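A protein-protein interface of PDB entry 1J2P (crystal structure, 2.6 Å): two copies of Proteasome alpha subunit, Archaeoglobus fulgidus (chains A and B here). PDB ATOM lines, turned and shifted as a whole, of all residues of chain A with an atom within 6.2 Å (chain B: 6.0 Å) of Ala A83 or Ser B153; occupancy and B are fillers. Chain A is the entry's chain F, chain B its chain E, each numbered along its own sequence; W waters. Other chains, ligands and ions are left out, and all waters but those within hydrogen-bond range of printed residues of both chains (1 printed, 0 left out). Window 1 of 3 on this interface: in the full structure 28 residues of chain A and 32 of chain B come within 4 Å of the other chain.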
ATOM      1  N   GLY A  80      -4.989  -6.093 -30.141  1.00  0.00           N
ATOM      2  CA  GLY A  80      -5.559  -6.872 -29.052  1.00  0.00           C
ATOM      3  C   GLY A  80      -4.481  -7.386 -28.105  1.00  0.00           C
ATOM      4  O   GLY A  80      -3.416  -6.784 -27.996  1.00  0.00           O
ATOM      5  N   LEU A  81      -4.748  -8.490 -27.414  1.00  0.00           N
ATOM      6  CA  LEU A  81      -3.768  -9.072 -26.486  1.00  0.00           C
ATOM      7  C   LEU A  81      -2.454  -9.357 -27.211  1.00  0.00           C
ATOM      8  O   LEU A  81      -2.439 -10.038 -28.222  1.00  0.00           O
ATOM      9  CB  LEU A  81      -4.321 -10.361 -25.867  1.00  0.00           C
ATOM     10  CG  LEU A  81      -5.588 -10.179 -25.026  1.00  0.00           C
ATOM     11  CD1 LEU A  81      -6.032 -11.526 -24.478  1.00  0.00           C
ATOM     12  CD2 LEU A  81      -5.328  -9.181 -23.902  1.00  0.00           C
ATOM     13  N   VAL A  82      -1.360  -8.833 -26.668  1.00  0.00           N
ATOM     14  CA  VAL A  82      -0.024  -8.963 -27.256  1.00  0.00           C
ATOM     15  C   VAL A  82       0.470 -10.381 -27.493  1.00  0.00           C
ATOM     16  O   VAL A  82       0.775 -10.741 -28.623  1.00  0.00           O
ATOM     17  CB  VAL A  82       1.024  -8.208 -26.399  1.00  0.00           C
ATOM     18  CG1 VAL A  82       2.420  -8.420 -26.962  1.00  0.00           C
ATOM     19  CG2 VAL A  82       0.704  -6.727 -26.386  1.00  0.00           C
ATOM     20  N   ALA A  83       0.561 -11.171 -26.426  1.00  0.00           N
ATOM     21  CA  ALA A  83       1.010 -12.557 -26.534  1.00  0.00           C
ATOM     22  C   ALA A  83       0.128 -13.355 -27.511  1.00  0.00           C
ATOM     23  O   ALA A  83       0.643 -14.115 -28.333  1.00  0.00           O
ATOM     24  CB  ALA A  83       1.012 -13.213 -25.162  1.00  0.00           C
ATOM     25  N   ASP A  84      -1.189 -13.174 -27.425  1.00  0.00           N
ATOM     26  CA  ASP A  84      -2.108 -13.871 -28.318  1.00  0.00           C
ATOM     27  C   ASP A  84      -1.772 -13.539 -29.776  1.00  0.00           C
ATOM     28  O   ASP A  84      -1.750 -14.410 -30.645  1.00  0.00           O
ATOM     29  CB  ASP A  84      -3.564 -13.451 -28.049  1.00  0.00           C
ATOM     30  CG  ASP A  84      -4.215 -14.214 -26.898  1.00  0.00           C
ATOM     31  OD1 ASP A  84      -5.442 -14.043 -26.710  1.00  0.00           O
ATOM     32  OD2 ASP A  84      -3.525 -14.985 -26.183  1.00  0.00           O
ATOM     33  N   ALA A  85      -1.514 -12.268 -30.042  1.00  0.00           N
ATOM     34  CA  ALA A  85      -1.208 -11.832 -31.396  1.00  0.00           C
ATOM     35  C   ALA A  85       0.039 -12.498 -31.970  1.00  0.00           C
ATOM     36  O   ALA A  85       0.011 -12.997 -33.092  1.00  0.00           O
ATOM     37  CB  ALA A  85      -1.055 -10.325 -31.427  1.00  0.00           C
ATOM     38  N   ARG A  86       1.122 -12.503 -31.197  1.00  0.00           N
ATOM     39  CA  ARG A  86       2.376 -13.089 -31.633  1.00  0.00           C
ATOM     40  C   ARG A  86       2.151 -14.543 -32.030  1.00  0.00           C
ATOM     41  O   ARG A  86       2.600 -14.984 -33.083  1.00  0.00           O
ATOM     42  CB  ARG A  86       3.421 -12.986 -30.514  1.00  0.00           C
ATOM     43  CG  ARG A  86       4.852 -13.298 -30.956  1.00  0.00           C
ATOM     44  CD  ARG A  86       5.843 -13.318 -29.778  1.00  0.00           C
ATOM     45  NE  ARG A  86       5.472 -14.311 -28.767  1.00  0.00           N
ATOM     46  CZ  ARG A  86       4.970 -14.015 -27.572  1.00  0.00           C
ATOM     47  NH1 ARG A  86       4.783 -12.739 -27.217  1.00  0.00           N
ATOM     48  NH2 ARG A  86       4.629 -14.996 -26.744  1.00  0.00           N
ATOM     49  N   VAL A  87       1.428 -15.278 -31.192  1.00  0.00           N
ATOM     50  CA  VAL A  87       1.144 -16.684 -31.444  1.00  0.00           C
ATOM     51  C   VAL A  87       0.401 -16.871 -32.753  1.00  0.00           C
ATOM     52  O   VAL A  87       0.669 -17.792 -33.504  1.00  0.00           O
ATOM     53  CB  VAL A  87       0.325 -17.283 -30.277  1.00  0.00           C
ATOM     54  CG1 VAL A  87      -0.213 -18.658 -30.639  1.00  0.00           C
ATOM     55  CG2 VAL A  87       1.208 -17.384 -29.048  1.00  0.00           C
ATOM     56  N   LEU A  88      -0.532 -15.978 -33.030  1.00  0.00           N
ATOM     57  CA  LEU A  88      -1.307 -16.045 -34.259  1.00  0.00           C
ATOM     58  C   LEU A  88      -0.426 -15.798 -35.490  1.00  0.00           C
ATOM     59  O   LEU A  88      -0.593 -16.454 -36.524  1.00  0.00           O
ATOM     60  CB  LEU A  88      -2.449 -15.020 -34.197  1.00  0.00           C
ATOM     61  CG  LEU A  88      -3.898 -15.513 -34.042  1.00  0.00           C
ATOM     62  CD1 LEU A  88      -3.958 -16.878 -33.404  1.00  0.00           C
ATOM     63  CD2 LEU A  88      -4.670 -14.508 -33.223  1.00  0.00           C
ATOM     64  N   VAL B  24      -4.605 -12.681 -15.138  1.00  0.00           N
ATOM     65  CA  VAL B  24      -3.282 -12.317 -15.630  1.00  0.00           C
ATOM     66  C   VAL B  24      -2.851 -11.039 -14.899  1.00  0.00           C
ATOM     67  O   VAL B  24      -1.689 -10.887 -14.508  1.00  0.00           O
ATOM     68  CB  VAL B  24      -3.283 -12.044 -17.170  1.00  0.00           C
ATOM     69  CG1 VAL B  24      -2.026 -11.281 -17.564  1.00  0.00           C
ATOM     70  CG2 VAL B  24      -3.350 -13.357 -17.944  1.00  0.00           C
ATOM     71  N   ARG B  28       0.303 -10.536 -12.333  1.00  0.00           N
ATOM     72  CA  ARG B  28       1.266  -9.441 -12.379  1.00  0.00           C
ATOM     73  C   ARG B  28       1.504  -8.843 -10.990  1.00  0.00           C
ATOM     74  O   ARG B  28       2.577  -8.284 -10.720  1.00  0.00           O
ATOM     75  CB  ARG B  28       0.807  -8.354 -13.365  1.00  0.00           C
ATOM     76  CG  ARG B  28       0.795  -8.845 -14.799  1.00  0.00           C
ATOM     77  CD  ARG B  28       0.973  -7.723 -15.808  1.00  0.00           C
ATOM     78  NE  ARG B  28      -0.301  -7.254 -16.318  1.00  0.00           N
ATOM     79  CZ  ARG B  28      -0.771  -7.489 -17.536  1.00  0.00           C
ATOM     80  NH1 ARG B  28      -0.069  -8.199 -18.413  1.00  0.00           N
ATOM     81  NH2 ARG B  28      -1.958  -7.011 -17.867  1.00  0.00           N
ATOM     82  N   CYS B 117       8.133 -17.033 -23.992  1.00  0.00           N
ATOM     83  CA  CYS B 117       6.893 -16.272 -23.937  1.00  0.00           C
ATOM     84  C   CYS B 117       5.741 -16.995 -24.606  1.00  0.00           C
ATOM     85  O   CYS B 117       4.589 -16.805 -24.221  1.00  0.00           O
ATOM     86  CB  CYS B 117       7.066 -14.885 -24.555  1.00  0.00           C
ATOM     87  SG  CYS B 117       7.951 -13.720 -23.482  1.00  0.00           S
ATOM     88  N   ASP B 118       6.030 -17.824 -25.605  1.00  0.00           N
ATOM     89  CA  ASP B 118       4.951 -18.556 -26.263  1.00  0.00           C
ATOM     90  C   ASP B 118       4.495 -19.622 -25.281  1.00  0.00           C
ATOM     91  O   ASP B 118       3.330 -20.020 -25.247  1.00  0.00           O
ATOM     92  CB  ASP B 118       5.419 -19.240 -27.552  1.00  0.00           C
ATOM     93  CG  ASP B 118       5.740 -18.258 -28.655  1.00  0.00           C
ATOM     94  OD1 ASP B 118       5.083 -17.197 -28.727  1.00  0.00           O
ATOM     95  OD2 ASP B 118       6.645 -18.562 -29.464  1.00  0.00           O
ATOM     96  N   LYS B 120       4.590 -19.294 -21.974  1.00  0.00           N
ATOM     97  CA  LYS B 120       3.792 -18.631 -20.960  1.00  0.00           C
ATOM     98  C   LYS B 120       2.405 -18.277 -21.480  1.00  0.00           C
ATOM     99  O   LYS B 120       1.426 -18.357 -20.756  1.00  0.00           O
ATOM    100  CB  LYS B 120       4.527 -17.381 -20.457  1.00  0.00           C
ATOM    101  CG  LYS B 120       5.672 -17.718 -19.505  1.00  0.00           C
ATOM    102  CD  LYS B 120       6.699 -16.611 -19.429  1.00  0.00           C
ATOM    103  CE  LYS B 120       6.233 -15.451 -18.579  1.00  0.00           C
ATOM    104  NZ  LYS B 120       7.293 -14.395 -18.502  1.00  0.00           N
ATOM    105  N   GLN B 121       2.324 -17.909 -22.752  1.00  0.00           N
ATOM    106  CA  GLN B 121       1.053 -17.541 -23.352  1.00  0.00           C
ATOM    107  C   GLN B 121       0.065 -18.704 -23.284  1.00  0.00           C
ATOM    108  O   GLN B 121      -1.126 -18.510 -23.043  1.00  0.00           O
ATOM    109  CB  GLN B 121       1.272 -17.108 -24.805  1.00  0.00           C
ATOM    110  CG  GLN B 121       0.030 -16.531 -25.478  1.00  0.00           C
ATOM    111  CD  GLN B 121      -0.958 -17.589 -25.944  1.00  0.00           C
ATOM    112  OE1 GLN B 121      -2.114 -17.275 -26.227  1.00  0.00           O
ATOM    113  NE2 GLN B 121      -0.512 -18.835 -26.038  1.00  0.00           N
ATOM    114  N   GLN B 122       0.565 -19.915 -23.481  1.00  0.00           N
ATOM    115  CA  GLN B 122      -0.291 -21.088 -23.436  1.00  0.00           C
ATOM    116  C   GLN B 122      -0.878 -21.362 -22.050  1.00  0.00           C
ATOM    117  O   GLN B 122      -1.969 -21.912 -21.942  1.00  0.00           O
ATOM    118  CB  GLN B 122       0.472 -22.313 -23.946  1.00  0.00           C
ATOM    119  CG  GLN B 122       0.702 -22.308 -25.458  1.00  0.00           C
ATOM    120  CD  GLN B 122      -0.605 -22.338 -26.281  1.00  0.00           C
ATOM    121  OE1 GLN B 122      -1.399 -21.381 -26.280  1.00  0.00           O
ATOM    122  NE2 GLN B 122      -0.824 -23.450 -26.989  1.00  0.00           N
ATOM    123  N   THR B 124      -2.160 -19.516 -20.403  1.00  0.00           N
ATOM    124  CA  THR B 124      -3.068 -18.394 -20.290  1.00  0.00           C
ATOM    125  C   THR B 124      -4.401 -18.630 -20.983  1.00  0.00           C
ATOM    126  O   THR B 124      -5.346 -17.875 -20.783  1.00  0.00           O
ATOM    127  CB  THR B 124      -2.357 -17.149 -20.847  1.00  0.00           C
ATOM    128  OG1 THR B 124      -2.032 -16.269 -19.766  1.00  0.00           O
ATOM    129  CG2 THR B 124      -3.180 -16.453 -21.887  1.00  0.00           C
ATOM    130  N   PHE B 132       2.067 -18.424 -15.126  1.00  0.00           N
ATOM    131  CA  PHE B 132       3.294 -18.257 -14.335  1.00  0.00           C
ATOM    132  C   PHE B 132       3.268 -16.868 -13.709  1.00  0.00           C
ATOM    133  O   PHE B 132       3.039 -15.883 -14.402  1.00  0.00           O
ATOM    134  CB  PHE B 132       4.546 -18.384 -15.214  1.00  0.00           C
ATOM    135  CG  PHE B 132       4.845 -19.785 -15.642  1.00  0.00           C
ATOM    136  CD1 PHE B 132       4.326 -20.291 -16.824  1.00  0.00           C
ATOM    137  CD2 PHE B 132       5.628 -20.608 -14.849  1.00  0.00           C
ATOM    138  CE1 PHE B 132       4.580 -21.602 -17.213  1.00  0.00           C
ATOM    139  CE2 PHE B 132       5.891 -21.918 -15.222  1.00  0.00           C
ATOM    140  CZ  PHE B 132       5.365 -22.422 -16.410  1.00  0.00           C
ATOM    141  N   ASP B 151       6.270 -10.886 -19.564  1.00  0.00           N
ATOM    142  CA  ASP B 151       5.096 -10.666 -18.758  1.00  0.00           C
ATOM    143  C   ASP B 151       4.398 -12.006 -18.467  1.00  0.00           C
ATOM    144  O   ASP B 151       4.534 -12.960 -19.218  1.00  0.00           O
ATOM    145  CB  ASP B 151       4.177  -9.733 -19.547  1.00  0.00           C
ATOM    146  CG  ASP B 151       2.816  -9.627 -18.952  1.00  0.00           C
ATOM    147  OD1 ASP B 151       2.677  -8.920 -17.942  1.00  0.00           O
ATOM    148  OD2 ASP B 151       1.887 -10.259 -19.492  1.00  0.00           O
ATOM    149  N   PRO B 152       3.657 -12.098 -17.357  1.00  0.00           N
ATOM    150  CA  PRO B 152       2.966 -13.360 -17.051  1.00  0.00           C
ATOM    151  C   PRO B 152       2.062 -13.826 -18.199  1.00  0.00           C
ATOM    152  O   PRO B 152       1.856 -15.015 -18.387  1.00  0.00           O
ATOM    153  CB  PRO B 152       2.167 -13.014 -15.794  1.00  0.00           C
ATOM    154  CG  PRO B 152       3.066 -12.042 -15.091  1.00  0.00           C
ATOM    155  CD  PRO B 152       3.562 -11.153 -16.228  1.00  0.00           C
ATOM    156  N   SER B 153       1.520 -12.891 -18.973  1.00  0.00           N
ATOM    157  CA  SER B 153       0.642 -13.253 -20.083  1.00  0.00           C
ATOM    158  C   SER B 153       1.404 -13.761 -21.317  1.00  0.00           C
ATOM    159  O   SER B 153       0.810 -14.326 -22.240  1.00  0.00           O
ATOM    160  CB  SER B 153      -0.196 -12.057 -20.499  1.00  0.00           C
ATOM    161  OG  SER B 153       0.565 -11.225 -21.336  1.00  0.00           O
ATOM    162  N   GLY B 154       2.713 -13.538 -21.347  1.00  0.00           N
ATOM    163  CA  GLY B 154       3.496 -13.983 -22.480  1.00  0.00           C
ATOM    164  C   GLY B 154       3.875 -12.849 -23.410  1.00  0.00           C
ATOM    165  O   GLY B 154       4.488 -13.074 -24.455  1.00  0.00           O
ATOM    166  N   ALA B 155       3.486 -11.629 -23.054  1.00  0.00           N
ATOM    167  CA  ALA B 155       3.834 -10.462 -23.860  1.00  0.00           C
ATOM    168  C   ALA B 155       5.355 -10.315 -23.824  1.00  0.00           C
ATOM    169  O   ALA B 155       6.006 -10.682 -22.845  1.00  0.00           O
ATOM    170  CB  ALA B 155       3.175  -9.210 -23.295  1.00  0.00           C
ATOM    171  N   LEU B 156       5.912  -9.777 -24.897  1.00  0.00           N
ATOM    172  CA  LEU B 156       7.350  -9.607 -25.010  1.00  0.00           C
ATOM    173  C   LEU B 156       7.660  -8.219 -25.541  1.00  0.00           C
ATOM    174  O   LEU B 156       7.081  -7.787 -26.533  1.00  0.00           O
ATOM    175  CB  LEU B 156       7.915 -10.666 -25.961  1.00  0.00           C
ATOM    176  CG  LEU B 156       9.413 -10.624 -26.251  1.00  0.00           C
ATOM    177  CD1 LEU B 156      10.189 -10.746 -24.962  1.00  0.00           C
ATOM    178  CD2 LEU B 156       9.771 -11.763 -27.209  1.00  0.00           C
HETATM  179  O   HOH W   1       5.152  -9.717 -28.015  1.00  0.00           O
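Of chain B, only Gln B121, Ser B153, Gly B154 and Ala B155 come within 4 Å of Ala A83.
Ser B153 touches just one residue of chain A: Ala A83.
Of the printed residues of chain B, Val A87 touches Asp B118 (3.9 Å) and Gln B121 (3.8 Å).
Printed residues of chain B within 4 Å of Val A82: Ala B155 (3.8 Å).
Of the printed residues of chain A, Ala B155 touches Val A82 and Ala A83.
Of the printed residues of chain A, Leu B156 touches Arg A86.
Val B24 touches none of the printed residues of chain A.
Asp B151 touches none of the printed residues of chain A.
The nearest residue of chain B that does not touch Ala A83 is Cys B117 (5.2 Å).
The nearest residue of chain A that does not touch Ser B153 is Asp A84 (5.7 Å).
The nearest printed residue of chain A that does not touch Gly B154 is Val A82 (5.7 Å).
No position is printed for both chains.
Of the 12 pairs that touch across the chains among the printed residues, none has its exchanged pair printed and touching as well.
The backbone carbonyl oxygen (O) of Cys B117 is in hydrogen-bond range of the guanidinium group (NH2) of Arg A86.
NH1 of Arg A86 lies within hydrogen-bond range of O of Gly B154.
The side-chain amide oxygen (OE1) of Gln B121 lies close to the side-chain carboxylate (OD2) of Asp A84 (2.7 Å).
The side-chain carboxylate (OD1) of Asp B118 lies within salt-bridge range of the guanidinium group (NE) of Arg A86 (2.9 Å).
Of the 9 printed residues of chain A, 5 touch a printed residue of chain B.
Printed residues of chain A that touch a printed residue of chain B: Val A82, Ala A83, Asp A84, Arg A86 and Val A87.
Printed residues of chain B that touch a printed residue of chain A: Cys B117, Asp B118, Gln B121, Ser B153, Gly B154, Ala B155 and Leu B156.
Among the printed residues, 12 pairs touch across the chains.
Among the printed residues, Asp or Glu carboxylates within 4 Å of a Lys or Arg side-chain nitrogen of the other chain: Arg A86 with Asp B118 (2.9 Å).
Water W1 bridges the backbone carbonyl oxygen of Leu B156 (3.1 Å) and the guanidinium group of Arg A86 (3.1 Å).
Val A82 touches Ala B155 (CG1 to CB, 3.8 Å).
Ala A83 touches Gln B121 (CB to CG, 3.5 Å).
Ser B153 touches Ala A83.
Ala A83 touches Gly B154 (CB to C, 3.4 Å).
Ala A83 touches Ala B155.
Arg A86 touches Leu B156 (NH1 to N, 3.9 Å).
Val A87 touches Asp B118 (CG2 to OD1, 3.9 Å).
Val A87 touches Gln B121 (CG2 to NE2, 3.8 Å).
OD2 of Asp B151 sits at hydrogen-bond distance from OG of Ser B153 (2.5 Å).
The backbone carbonyl oxygen (O) of Ala B155 is in hydrogen-bond range of the side-chain sulfur (SG) of Cys B117, 3.7 Å away.
OG of Ser B153 lies within hydrogen-bond range of N of Ala B155.
The side-chain amide oxygen (OE1) of Gln B122 sits at hydrogen-bond distance from the side-chain amide nitrogen (NE2) of Gln B121.
The side-chain sulfur (SG) of Cys B117 sits close to the backbone carbonyl oxygen (O) of Gly B154 (3.7 Å).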
